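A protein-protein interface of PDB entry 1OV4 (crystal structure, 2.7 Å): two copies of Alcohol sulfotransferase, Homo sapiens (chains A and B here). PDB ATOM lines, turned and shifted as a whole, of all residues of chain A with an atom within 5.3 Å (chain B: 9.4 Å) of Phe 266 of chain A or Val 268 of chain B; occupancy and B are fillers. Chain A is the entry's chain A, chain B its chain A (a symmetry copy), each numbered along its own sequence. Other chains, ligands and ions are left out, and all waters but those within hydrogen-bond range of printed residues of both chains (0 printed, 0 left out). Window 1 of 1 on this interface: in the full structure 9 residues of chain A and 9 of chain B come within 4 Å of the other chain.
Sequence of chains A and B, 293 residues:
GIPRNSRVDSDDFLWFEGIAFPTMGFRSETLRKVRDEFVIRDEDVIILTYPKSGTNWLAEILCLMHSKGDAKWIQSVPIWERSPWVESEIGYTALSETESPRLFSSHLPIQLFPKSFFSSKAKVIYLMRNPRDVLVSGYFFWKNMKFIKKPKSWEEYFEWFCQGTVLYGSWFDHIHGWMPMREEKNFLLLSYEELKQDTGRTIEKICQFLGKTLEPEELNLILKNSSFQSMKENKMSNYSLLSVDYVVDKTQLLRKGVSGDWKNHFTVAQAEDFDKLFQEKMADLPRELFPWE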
ATOM      1  N   ARG A 132      20.924 -10.650  20.801  1.00  0.00           N
ATOM      2  CA  ARG A 132      20.967 -10.075  22.143  1.00  0.00           C
ATOM      3  C   ARG A 132      20.412 -11.067  23.155  1.00  0.00           C
ATOM      4  O   ARG A 132      20.965 -11.238  24.235  1.00  0.00           O
ATOM      5  CB  ARG A 132      20.147  -8.796  22.188  1.00  0.00           C
ATOM      6  CG  ARG A 132      20.596  -7.780  21.173  1.00  0.00           C
ATOM      7  CD  ARG A 132      19.602  -6.672  21.077  1.00  0.00           C
ATOM      8  NE  ARG A 132      20.018  -5.718  20.071  1.00  0.00           N
ATOM      9  CZ  ARG A 132      20.002  -5.962  18.769  1.00  0.00           C
ATOM     10  NH1 ARG A 132      19.572  -7.143  18.327  1.00  0.00           N
ATOM     11  NH2 ARG A 132      20.443  -5.037  17.917  1.00  0.00           N
ATOM     12  N   LEU A 135      22.800 -13.942  23.495  1.00  0.00           N
ATOM     13  CA  LEU A 135      23.929 -13.618  24.364  1.00  0.00           C
ATOM     14  C   LEU A 135      23.540 -13.778  25.852  1.00  0.00           C
ATOM     15  O   LEU A 135      24.275 -14.384  26.636  1.00  0.00           O
ATOM     16  CB  LEU A 135      24.390 -12.194  24.080  1.00  0.00           C
ATOM     17  CG  LEU A 135      25.611 -11.635  24.803  1.00  0.00           C
ATOM     18  CD1 LEU A 135      26.161 -10.440  24.032  1.00  0.00           C
ATOM     19  CD2 LEU A 135      25.223 -11.213  26.204  1.00  0.00           C
ATOM     20  N   VAL A 136      22.381 -13.233  26.217  1.00  0.00           N
ATOM     21  CA  VAL A 136      21.873 -13.308  27.573  1.00  0.00           C
ATOM     22  C   VAL A 136      21.679 -14.757  27.986  1.00  0.00           C
ATOM     23  O   VAL A 136      22.096 -15.185  29.072  1.00  0.00           O
ATOM     24  CB  VAL A 136      20.515 -12.604  27.710  1.00  0.00           C
ATOM     25  CG1 VAL A 136      19.917 -12.899  29.085  1.00  0.00           C
ATOM     26  CG2 VAL A 136      20.695 -11.110  27.501  1.00  0.00           C
ATOM     27  N   TRP A 154      29.806 -10.286  33.469  1.00  0.00           N
ATOM     28  CA  TRP A 154      28.905  -9.991  32.364  1.00  0.00           C
ATOM     29  C   TRP A 154      29.616  -9.130  31.337  1.00  0.00           C
ATOM     30  O   TRP A 154      29.534  -9.382  30.137  1.00  0.00           O
ATOM     31  CB  TRP A 154      27.667  -9.278  32.899  1.00  0.00           C
ATOM     32  CG  TRP A 154      26.905  -8.508  31.887  1.00  0.00           C
ATOM     33  CD1 TRP A 154      26.946  -7.165  31.687  1.00  0.00           C
ATOM     34  CD2 TRP A 154      25.976  -9.030  30.930  1.00  0.00           C
ATOM     35  NE1 TRP A 154      26.100  -6.810  30.664  1.00  0.00           N
ATOM     36  CE2 TRP A 154      25.497  -7.935  30.180  1.00  0.00           C
ATOM     37  CE3 TRP A 154      25.512 -10.315  30.629  1.00  0.00           C
ATOM     38  CZ2 TRP A 154      24.561  -8.087  29.148  1.00  0.00           C
ATOM     39  CZ3 TRP A 154      24.587 -10.467  29.603  1.00  0.00           C
ATOM     40  CH2 TRP A 154      24.123  -9.356  28.871  1.00  0.00           C
ATOM     41  N   PHE A 158      30.128 -10.435  27.426  1.00  0.00           N
ATOM     42  CA  PHE A 158      29.581  -9.570  26.396  1.00  0.00           C
ATOM     43  C   PHE A 158      30.657  -9.366  25.349  1.00  0.00           C
ATOM     44  O   PHE A 158      30.440  -9.577  24.153  1.00  0.00           O
ATOM     45  CB  PHE A 158      29.203  -8.210  26.986  1.00  0.00           C
ATOM     46  CG  PHE A 158      28.578  -7.272  25.995  1.00  0.00           C
ATOM     47  CD1 PHE A 158      27.211  -7.321  25.732  1.00  0.00           C
ATOM     48  CD2 PHE A 158      29.357  -6.338  25.317  1.00  0.00           C
ATOM     49  CE1 PHE A 158      26.628  -6.451  24.808  1.00  0.00           C
ATOM     50  CE2 PHE A 158      28.783  -5.462  24.389  1.00  0.00           C
ATOM     51  CZ  PHE A 158      27.417  -5.519  24.137  1.00  0.00           C
ATOM     52  N   TRP A 262      16.479  -9.445  27.131  1.00  0.00           N
ATOM     53  CA  TRP A 262      17.831  -8.894  26.999  1.00  0.00           C
ATOM     54  C   TRP A 262      17.953  -7.466  27.549  1.00  0.00           C
ATOM     55  O   TRP A 262      19.007  -7.064  28.053  1.00  0.00           O
ATOM     56  CB  TRP A 262      18.305  -8.923  25.544  1.00  0.00           C
ATOM     57  CG  TRP A 262      17.618  -7.964  24.633  1.00  0.00           C
ATOM     58  CD1 TRP A 262      16.515  -8.210  23.869  1.00  0.00           C
ATOM     59  CD2 TRP A 262      18.031  -6.624  24.328  1.00  0.00           C
ATOM     60  NE1 TRP A 262      16.216  -7.107  23.096  1.00  0.00           N
ATOM     61  CE2 TRP A 262      17.121  -6.116  23.367  1.00  0.00           C
ATOM     62  CE3 TRP A 262      19.067  -5.798  24.786  1.00  0.00           C
ATOM     63  CZ2 TRP A 262      17.237  -4.822  22.830  1.00  0.00           C
ATOM     64  CZ3 TRP A 262      19.184  -4.507  24.252  1.00  0.00           C
ATOM     65  CH2 TRP A 262      18.265  -4.031  23.291  1.00  0.00           C
ATOM     66  N   LYS A 263      16.865  -6.709  27.459  1.00  0.00           N
ATOM     67  CA  LYS A 263      16.841  -5.332  27.941  1.00  0.00           C
ATOM     68  C   LYS A 263      17.087  -5.238  29.441  1.00  0.00           C
ATOM     69  O   LYS A 263      17.499  -4.190  29.952  1.00  0.00           O
ATOM     70  CB  LYS A 263      15.512  -4.683  27.576  1.00  0.00           C
ATOM     71  CG  LYS A 263      15.385  -4.450  26.086  1.00  0.00           C
ATOM     72  CD  LYS A 263      14.087  -3.759  25.744  1.00  0.00           C
ATOM     73  CE  LYS A 263      14.068  -3.330  24.298  1.00  0.00           C
ATOM     74  NZ  LYS A 263      12.800  -2.625  24.018  1.00  0.00           N
ATOM     75  N   ASN A 264      16.841  -6.333  30.146  1.00  0.00           N
ATOM     76  CA  ASN A 264      17.079  -6.352  31.573  1.00  0.00           C
ATOM     77  C   ASN A 264      18.549  -6.593  31.853  1.00  0.00           C
ATOM     78  O   ASN A 264      18.947  -6.653  33.011  1.00  0.00           O
ATOM     79  CB  ASN A 264      16.289  -7.463  32.239  1.00  0.00           C
ATOM     80  CG  ASN A 264      14.820  -7.221  32.205  1.00  0.00           C
ATOM     81  OD1 ASN A 264      14.336  -6.181  32.652  1.00  0.00           O
ATOM     82  ND2 ASN A 264      14.084  -8.185  31.681  1.00  0.00           N
ATOM     83  N   HIS A 265      19.363  -6.733  30.810  1.00  0.00           N
ATOM     84  CA  HIS A 265      20.778  -7.001  31.030  1.00  0.00           C
ATOM     85  C   HIS A 265      21.773  -6.106  30.301  1.00  0.00           C
ATOM     86  O   HIS A 265      22.818  -5.777  30.853  1.00  0.00           O
ATOM     87  CB  HIS A 265      21.035  -8.465  30.720  1.00  0.00           C
ATOM     88  CG  HIS A 265      20.199  -9.395  31.545  1.00  0.00           C
ATOM     89  ND1 HIS A 265      20.577  -9.825  32.803  1.00  0.00           N
ATOM     90  CD2 HIS A 265      18.971  -9.926  31.322  1.00  0.00           C
ATOM     91  CE1 HIS A 265      19.621 -10.578  33.316  1.00  0.00           C
ATOM     92  NE2 HIS A 265      18.635 -10.655  32.439  1.00  0.00           N
ATOM     93  N   PHE A 266      21.469  -5.712  29.068  1.00  0.00           N
ATOM     94  CA  PHE A 266      22.381  -4.830  28.344  1.00  0.00           C
ATOM     95  C   PHE A 266      22.244  -3.457  28.940  1.00  0.00           C
ATOM     96  O   PHE A 266      21.127  -3.031  29.240  1.00  0.00           O
ATOM     97  CB  PHE A 266      21.995  -4.698  26.873  1.00  0.00           C
ATOM     98  CG  PHE A 266      22.387  -5.862  26.025  1.00  0.00           C
ATOM     99  CD1 PHE A 266      22.038  -7.156  26.387  1.00  0.00           C
ATOM    100  CD2 PHE A 266      23.073  -5.658  24.832  1.00  0.00           C
ATOM    101  CE1 PHE A 266      22.367  -8.229  25.573  1.00  0.00           C
ATOM    102  CE2 PHE A 266      23.404  -6.721  24.015  1.00  0.00           C
ATOM    103  CZ  PHE A 266      23.049  -8.008  24.385  1.00  0.00           C
ATOM    104  N   THR A 267      23.355  -2.764  29.140  1.00  0.00           N
ATOM    105  CA  THR A 267      23.234  -1.405  29.633  1.00  0.00           C
ATOM    106  C   THR A 267      22.884  -0.638  28.369  1.00  0.00           C
ATOM    107  O   THR A 267      22.974  -1.188  27.277  1.00  0.00           O
ATOM    108  CB  THR A 267      24.541  -0.870  30.240  1.00  0.00           C
ATOM    109  OG1 THR A 267      25.604  -0.997  29.288  1.00  0.00           O
ATOM    110  CG2 THR A 267      24.889  -1.648  31.511  1.00  0.00           C
ATOM    111  N   VAL A 268      22.458   0.610  28.509  1.00  0.00           N
ATOM    112  CA  VAL A 268      22.087   1.405  27.344  1.00  0.00           C
ATOM    113  C   VAL A 268      23.263   1.539  26.404  1.00  0.00           C
ATOM    114  O   VAL A 268      23.091   1.597  25.188  1.00  0.00           O
ATOM    115  CB  VAL A 268      21.571   2.811  27.742  1.00  0.00           C
ATOM    116  CG1 VAL A 268      21.275   3.622  26.493  1.00  0.00           C
ATOM    117  CG2 VAL A 268      20.312   2.664  28.598  1.00  0.00           C
ATOM    118  N   GLN A 270      25.698  -0.700  25.955  1.00  0.00           N
ATOM    119  CA  GLN A 270      25.967  -1.956  25.275  1.00  0.00           C
ATOM    120  C   GLN A 270      25.001  -2.137  24.118  1.00  0.00           C
ATOM    121  O   GLN A 270      25.358  -2.691  23.080  1.00  0.00           O
ATOM    122  CB  GLN A 270      25.854  -3.104  26.274  1.00  0.00           C
ATOM    123  CG  GLN A 270      26.858  -2.968  27.398  1.00  0.00           C
ATOM    124  CD  GLN A 270      26.744  -4.039  28.432  1.00  0.00           C
ATOM    125  OE1 GLN A 270      25.666  -4.296  28.965  1.00  0.00           O
ATOM    126  NE2 GLN A 270      27.862  -4.669  28.741  1.00  0.00           N
ATOM    127  N   ALA A 271      23.776  -1.657  24.302  1.00  0.00           N
ATOM    128  CA  ALA A 271      22.751  -1.748  23.272  1.00  0.00           C
ATOM    129  C   ALA A 271      23.165  -0.920  22.050  1.00  0.00           C
ATOM    130  O   ALA A 271      23.119  -1.395  20.915  1.00  0.00           O
ATOM    131  CB  ALA A 271      21.418  -1.257  23.828  1.00  0.00           C
ATOM    132  N   PHE A 274      26.092  -2.475  20.588  1.00  0.00           N
ATOM    133  CA  PHE A 274      25.704  -3.676  19.900  1.00  0.00           C
ATOM    134  C   PHE A 274      25.033  -3.323  18.582  1.00  0.00           C
ATOM    135  O   PHE A 274      25.336  -3.927  17.547  1.00  0.00           O
ATOM    136  CB  PHE A 274      24.765  -4.540  20.727  1.00  0.00           C
ATOM    137  CG  PHE A 274      24.662  -5.943  20.201  1.00  0.00           C
ATOM    138  CD1 PHE A 274      25.688  -6.866  20.443  1.00  0.00           C
ATOM    139  CD2 PHE A 274      23.581  -6.331  19.413  1.00  0.00           C
ATOM    140  CE1 PHE A 274      25.643  -8.158  19.907  1.00  0.00           C
ATOM    141  CE2 PHE A 274      23.524  -7.619  18.871  1.00  0.00           C
ATOM    142  CZ  PHE A 274      24.559  -8.535  19.119  1.00  0.00           C
ATOM    143  N   TRP B 154      22.972  -1.974  43.049  1.00  0.00           N
ATOM    144  CA  TRP B 154      22.568  -0.960  42.086  1.00  0.00           C
ATOM    145  C   TRP B 154      21.069  -1.031  41.866  1.00  0.00           C
ATOM    146  O   TRP B 154      20.385  -0.009  41.852  1.00  0.00           O
ATOM    147  CB  TRP B 154      23.315  -1.181  40.776  1.00  0.00           C
ATOM    148  CG  TRP B 154      22.688  -0.557  39.587  1.00  0.00           C
ATOM    149  CD1 TRP B 154      21.928  -1.179  38.648  1.00  0.00           C
ATOM    150  CD2 TRP B 154      22.766   0.819  39.196  1.00  0.00           C
ATOM    151  NE1 TRP B 154      21.523  -0.280  37.691  1.00  0.00           N
ATOM    152  CE2 TRP B 154      22.019   0.953  38.006  1.00  0.00           C
ATOM    153  CE3 TRP B 154      23.384   1.949  39.741  1.00  0.00           C
ATOM    154  CZ2 TRP B 154      21.884   2.179  37.341  1.00  0.00           C
ATOM    155  CZ3 TRP B 154      23.247   3.166  39.084  1.00  0.00           C
ATOM    156  CH2 TRP B 154      22.498   3.272  37.896  1.00  0.00           C
ATOM    157  N   PHE B 158      18.620   2.218  42.709  1.00  0.00           N
ATOM    158  CA  PHE B 158      17.817   2.707  41.602  1.00  0.00           C
ATOM    159  C   PHE B 158      16.392   2.853  42.097  1.00  0.00           C
ATOM    160  O   PHE B 158      15.768   3.908  41.960  1.00  0.00           O
ATOM    161  CB  PHE B 158      17.837   1.706  40.445  1.00  0.00           C
ATOM    162  CG  PHE B 158      17.072   2.161  39.236  1.00  0.00           C
ATOM    163  CD1 PHE B 158      17.671   2.981  38.282  1.00  0.00           C
ATOM    164  CD2 PHE B 158      15.748   1.775  39.050  1.00  0.00           C
ATOM    165  CE1 PHE B 158      16.961   3.408  37.158  1.00  0.00           C
ATOM    166  CE2 PHE B 158      15.027   2.198  37.927  1.00  0.00           C
ATOM    167  CZ  PHE B 158      15.636   3.014  36.981  1.00  0.00           C
ATOM    168  N   TRP B 262      25.573   7.943  32.402  1.00  0.00           N
ATOM    169  CA  TRP B 262      24.483   7.130  32.948  1.00  0.00           C
ATOM    170  C   TRP B 262      24.166   5.897  32.090  1.00  0.00           C
ATOM    171  O   TRP B 262      23.754   4.851  32.602  1.00  0.00           O
ATOM    172  CB  TRP B 262      23.211   7.959  33.139  1.00  0.00           C
ATOM    173  CG  TRP B 262      22.528   8.375  31.881  1.00  0.00           C
ATOM    174  CD1 TRP B 262      22.715   9.539  31.196  1.00  0.00           C
ATOM    175  CD2 TRP B 262      21.488   7.663  31.194  1.00  0.00           C
ATOM    176  NE1 TRP B 262      21.850   9.605  30.124  1.00  0.00           N
ATOM    177  CE2 TRP B 262      21.095   8.462  30.091  1.00  0.00           C
ATOM    178  CE3 TRP B 262      20.865   6.422  31.390  1.00  0.00           C
ATOM    179  CZ2 TRP B 262      20.078   8.072  29.202  1.00  0.00           C
ATOM    180  CZ3 TRP B 262      19.852   6.031  30.505  1.00  0.00           C
ATOM    181  CH2 TRP B 262      19.478   6.852  29.418  1.00  0.00           C
ATOM    182  N   LYS B 263      24.372   6.025  30.784  1.00  0.00           N
ATOM    183  CA  LYS B 263      24.111   4.933  29.852  1.00  0.00           C
ATOM    184  C   LYS B 263      24.986   3.716  30.125  1.00  0.00           C
ATOM    185  O   LYS B 263      24.649   2.592  29.733  1.00  0.00           O
ATOM    186  CB  LYS B 263      24.307   5.421  28.421  1.00  0.00           C
ATOM    187  CG  LYS B 263      23.229   6.396  28.003  1.00  0.00           C
ATOM    188  CD  LYS B 263      23.405   6.832  26.567  1.00  0.00           C
ATOM    189  CE  LYS B 263      22.210   7.620  26.091  1.00  0.00           C
ATOM    190  NZ  LYS B 263      22.406   7.989  24.675  1.00  0.00           N
ATOM    191  N   ASN B 264      26.104   3.937  30.801  1.00  0.00           N
ATOM    192  CA  ASN B 264      26.982   2.837  31.140  1.00  0.00           C
ATOM    193  C   ASN B 264      26.466   2.119  32.372  1.00  0.00           C
ATOM    194  O   ASN B 264      27.084   1.161  32.822  1.00  0.00           O
ATOM    195  CB  ASN B 264      28.382   3.335  31.442  1.00  0.00           C
ATOM    196  CG  ASN B 264      29.069   3.877  30.236  1.00  0.00           C
ATOM    197  OD1 ASN B 264      29.189   3.202  29.215  1.00  0.00           O
ATOM    198  ND2 ASN B 264      29.540   5.107  30.340  1.00  0.00           N
ATOM    199  N   HIS B 265      25.343   2.570  32.926  1.00  0.00           N
ATOM    200  CA  HIS B 265      24.828   1.935  34.131  1.00  0.00           C
ATOM    201  C   HIS B 265      23.365   1.509  34.119  1.00  0.00           C
ATOM    202  O   HIS B 265      23.024   0.474  34.682  1.00  0.00           O
ATOM    203  CB  HIS B 265      25.119   2.850  35.308  1.00  0.00           C
ATOM    204  CG  HIS B 265      26.576   3.156  35.467  1.00  0.00           C
ATOM    205  ND1 HIS B 265      27.440   2.341  36.175  1.00  0.00           N
ATOM    206  CD2 HIS B 265      27.340   4.153  34.955  1.00  0.00           C
ATOM    207  CE1 HIS B 265      28.667   2.822  36.091  1.00  0.00           C
ATOM    208  NE2 HIS B 265      28.634   3.921  35.356  1.00  0.00           N
ATOM    209  N   PHE B 266      22.494   2.293  33.491  1.00  0.00           N
ATOM    210  CA  PHE B 266      21.086   1.909  33.430  1.00  0.00           C
ATOM    211  C   PHE B 266      20.971   0.789  32.434  1.00  0.00           C
ATOM    212  O   PHE B 266      21.613   0.839  31.383  1.00  0.00           O
ATOM    213  CB  PHE B 266      20.210   3.042  32.903  1.00  0.00           C
ATOM    214  CG  PHE B 266      19.914   4.110  33.903  1.00  0.00           C
ATOM    215  CD1 PHE B 266      20.937   4.728  34.609  1.00  0.00           C
ATOM    216  CD2 PHE B 266      18.605   4.532  34.108  1.00  0.00           C
ATOM    217  CE1 PHE B 266      20.660   5.749  35.505  1.00  0.00           C
ATOM    218  CE2 PHE B 266      18.319   5.549  34.998  1.00  0.00           C
ATOM    219  CZ  PHE B 266      19.349   6.160  35.696  1.00  0.00           C
ATOM    220  N   THR B 267      20.184  -0.230  32.748  1.00  0.00           N
ATOM    221  CA  THR B 267      19.994  -1.276  31.762  1.00  0.00           C
ATOM    222  C   THR B 267      18.961  -0.656  30.836  1.00  0.00           C
ATOM    223  O   THR B 267      18.389   0.378  31.165  1.00  0.00           O
ATOM    224  CB  THR B 267      19.454  -2.581  32.370  1.00  0.00           C
ATOM    225  OG1 THR B 267      18.251  -2.312  33.098  1.00  0.00           O
ATOM    226  CG2 THR B 267      20.497  -3.198  33.303  1.00  0.00           C
ATOM    227  N   VAL B 268      18.742  -1.256  29.674  1.00  0.00           N
ATOM    228  CA  VAL B 268      17.777  -0.713  28.724  1.00  0.00           C
ATOM    229  C   VAL B 268      16.403  -0.648  29.351  1.00  0.00           C
ATOM    230  O   VAL B 268      15.620   0.252  29.054  1.00  0.00           O
ATOM    231  CB  VAL B 268      17.720  -1.542  27.417  1.00  0.00           C
ATOM    232  CG1 VAL B 268      16.647  -0.981  26.501  1.00  0.00           C
ATOM    233  CG2 VAL B 268      19.086  -1.504  26.733  1.00  0.00           C
ATOM    234  N   ALA B 269      16.123  -1.593  30.236  1.00  0.00           N
ATOM    235  CA  ALA B 269      14.826  -1.657  30.892  1.00  0.00           C
ATOM    236  C   ALA B 269      14.644  -0.544  31.912  1.00  0.00           C
ATOM    237  O   ALA B 269      13.539  -0.021  32.082  1.00  0.00           O
ATOM    238  CB  ALA B 269      14.655  -2.991  31.554  1.00  0.00           C
ATOM    239  N   GLN B 270      15.727  -0.173  32.586  1.00  0.00           N
ATOM    240  CA  GLN B 270      15.659   0.882  33.583  1.00  0.00           C
ATOM    241  C   GLN B 270      15.465   2.226  32.904  1.00  0.00           C
ATOM    242  O   GLN B 270      14.784   3.106  33.429  1.00  0.00           O
ATOM    243  CB  GLN B 270      16.933   0.866  34.422  1.00  0.00           C
ATOM    244  CG  GLN B 270      17.101  -0.447  35.156  1.00  0.00           C
ATOM    245  CD  GLN B 270      18.367  -0.530  35.945  1.00  0.00           C
ATOM    246  OE1 GLN B 270      19.455  -0.284  35.428  1.00  0.00           O
ATOM    247  NE2 GLN B 270      18.242  -0.896  37.206  1.00  0.00           N
ATOM    248  N   ALA B 271      16.063   2.375  31.727  1.00  0.00           N
ATOM    249  CA  ALA B 271      15.952   3.606  30.957  1.00  0.00           C
ATOM    250  C   ALA B 271      14.496   3.823  30.529  1.00  0.00           C
ATOM    251  O   ALA B 271      13.936   4.906  30.705  1.00  0.00           O
ATOM    252  CB  ALA B 271      16.866   3.535  29.738  1.00  0.00           C
ATOM    253  N   GLU B 272      13.881   2.780  29.987  1.00  0.00           N
ATOM    254  CA  GLU B 272      12.498   2.863  29.537  1.00  0.00           C
ATOM    255  C   GLU B 272      11.583   3.097  30.722  1.00  0.00           C
ATOM    256  O   GLU B 272      10.652   3.898  30.643  1.00  0.00           O
ATOM    257  CB  GLU B 272      12.102   1.581  28.803  1.00  0.00           C
ATOM    258  CG  GLU B 272      13.030   1.239  27.642  1.00  0.00           C
ATOM    259  CD  GLU B 272      12.633  -0.039  26.928  1.00  0.00           C
ATOM    260  OE1 GLU B 272      11.976  -0.891  27.559  1.00  0.00           O
ATOM    261  OE2 GLU B 272      12.996  -0.202  25.746  1.00  0.00           O
ATOM    262  N   ASP B 273      11.839   2.396  31.822  1.00  0.00           N
ATOM    263  CA  ASP B 273      11.030   2.586  33.014  1.00  0.00           C
ATOM    264  C   ASP B 273      11.280   3.973  33.555  1.00  0.00           C
ATOM    265  O   ASP B 273      10.354   4.650  34.003  1.00  0.00           O
ATOM    266  CB  ASP B 273      11.380   1.576  34.087  1.00  0.00           C
ATOM    267  CG  ASP B 273      10.797   0.224  33.801  1.00  0.00           C
ATOM    268  OD1 ASP B 273       9.689   0.184  33.213  1.00  0.00           O
ATOM    269  OD2 ASP B 273      11.437  -0.787  34.176  1.00  0.00           O
ATOM    270  N   PHE B 274      12.531   4.413  33.514  1.00  0.00           N
ATOM    271  CA  PHE B 274      12.798   5.735  34.012  1.00  0.00           C
ATOM    272  C   PHE B 274      12.090   6.765  33.146  1.00  0.00           C
ATOM    273  O   PHE B 274      11.463   7.694  33.668  1.00  0.00           O
ATOM    274  CB  PHE B 274      14.285   6.050  34.053  1.00  0.00           C
ATOM    275  CG  PHE B 274      14.597   7.243  34.909  1.00  0.00           C
ATOM    276  CD1 PHE B 274      14.606   7.128  36.306  1.00  0.00           C
ATOM    277  CD2 PHE B 274      14.818   8.493  34.336  1.00  0.00           C
ATOM    278  CE1 PHE B 274      14.828   8.241  37.124  1.00  0.00           C
ATOM    279  CE2 PHE B 274      15.043   9.613  35.142  1.00  0.00           C
ATOM    280  CZ  PHE B 274      15.047   9.487  36.541  1.00  0.00           C
ATOM    281  N   ASP B 275      12.182   6.614  31.827  1.00  0.00           N
ATOM    282  CA  ASP B 275      11.522   7.566  30.942  1.00  0.00           C
ATOM    283  C   ASP B 275      10.054   7.649  31.317  1.00  0.00           C
ATOM    284  O   ASP B 275       9.542   8.722  31.636  1.00  0.00           O
ATOM    285  CB  ASP B 275      11.659   7.156  29.481  1.00  0.00           C
ATOM    286  CG  ASP B 275      13.062   7.376  28.946  1.00  0.00           C
ATOM    287  OD1 ASP B 275      13.663   8.423  29.277  1.00  0.00           O
ATOM    288  OD2 ASP B 275      13.561   6.513  28.186  1.00  0.00           O
ATOM    289  N   LYS B 276       9.385   6.502  31.304  1.00  0.00           N
ATOM    290  CA  LYS B 276       7.979   6.458  31.642  1.00  0.00           C
ATOM    291  C   LYS B 276       7.714   7.187  32.960  1.00  0.00           C
ATOM    292  O   LYS B 276       6.742   7.925  33.074  1.00  0.00           O
ATOM    293  CB  LYS B 276       7.517   5.002  31.721  1.00  0.00           C
ATOM    294  CG  LYS B 276       6.014   4.830  31.900  1.00  0.00           C
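Lys 263 of chain A touches four residues of chain B.
Of chain B, only Thr 267 (3.3 Å) and Val 268 (3.0 Å) come within 4 Å of Phe 266 of chain A.
Of chain B, only Lys 263, Asn 264, Phe 266, Thr 267 and Val 268 come within 4 Å of Thr 267 of chain A.
Of the printed residues of chain B, Val 268 of chain A touches Trp 262 (3.9 Å), Lys 263 (3.2 Å), Phe 266 (3.0 Å), Thr 267 (3.9 Å) and Ala 271 (3.7 Å).
Of chain A, only Trp 262, Lys 263, Phe 266, Thr 267 and Ala 271 come within 4 Å of Val 268 of chain B.
Printed residues of chain A within 4 Å of Ala 269 of chain B: Lys 263 and Asn 264.
Of the printed residues of chain A, Glu 272 of chain B touches Lys 263 (3.0 Å).
The backbone carbonyl oxygen of Lys 263 of chain A sits at hydrogen-bond distance from the backbone NH of Val 268 of chain B.
The backbone carbonyl oxygen (O) of Lys 263 of chain A sits at hydrogen-bond distance from the backbone NH (N) of Ala 269 of chain B (3.0 Å).
The side-chain carboxylate (OE2) of Glu 272 of chain B lies within salt-bridge range of the side-chain amino group (NZ) of Lys 263 of chain A, at 3.0 Å.
The backbone NH (N) of Val 268 of chain B is in hydrogen-bond range of the backbone carbonyl oxygen (O) of Phe 266 of chain A, 3.0 Å away.
The backbone carbonyl oxygen of Lys 263 of chain B is in hydrogen-bond range of the backbone NH of Val 268 of chain A (3.2 Å).
The backbone NH (N) of Val 268 of chain A lies within hydrogen-bond range of the backbone carbonyl oxygen (O) of Phe 266 of chain B (3.0 Å).
Val 268 of chain B touches Trp 262 of chain A.
Lys 263 of chain A touches Thr 267 of chain B.
Thr 267 of chain B touches Asn 264 of chain A.
Ala 269 of chain B touches Asn 264 of chain A (CB to OD1, 3.4 Å).
Lys 263 of chain B touches Thr 267 of chain A (O to CB, 3.5 Å).
O of Asn 264 of chain B touches CG2 of Thr 267 of chain A, at 3.8 Å.
CA of Thr 267 of chain A touches O of Phe 266 of chain B (3.3 Å).
CA of Thr 267 of chain A touches CA of Thr 267 of chain B, 3.9 Å away.
Thr 267 of chain B touches Val 268 of chain A (O to CG2, 3.9 Å).
Val 268 of chain A touches Ala 271 of chain B.
Of the 17 printed residues of chain B, 9 touch a printed residue of chain A.
Hydrophobic or aromatic side chains of chain A that line the printed part of chain B: Trp 262, Val 268 and Ala 271.
Among the printed residues, Asp or Glu carboxylates within 4 Å of a Lys or Arg side-chain nitrogen of the other chain: Lys 263 of chain A with Glu 272 of chain B (3.0 Å).
OE1 of Gln 270 of chain A is in hydrogen-bond range of N of Thr 267 of chain A (2.8 Å).
OE1 of Gln 270 of chain B is in hydrogen-bond range of N of Thr 267 of chain B, at 2.8 Å.
Trp 262 of chain A touches Val 268 of chain B, and with the chains exchanged Val 268 of chain A touches Trp 262 of chain B.
Phe 266 of chain A touches Thr 267 of chain B, and with the chains exchanged Thr 267 of chain A touches Phe 266 of chain B.
Thr 267 of chain A touches Val 268 of chain B, and with the chains exchanged Val 268 of chain A touches Thr 267 of chain B.
Val 268 of chain A touches Ala 271 of chain B, and with the chains exchanged Ala 271 of chain A touches Val 268 of chain B.
Of the 20 pairs that touch across the chains among the printed residues, 17 have their exchanged pair printed and touching as well.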
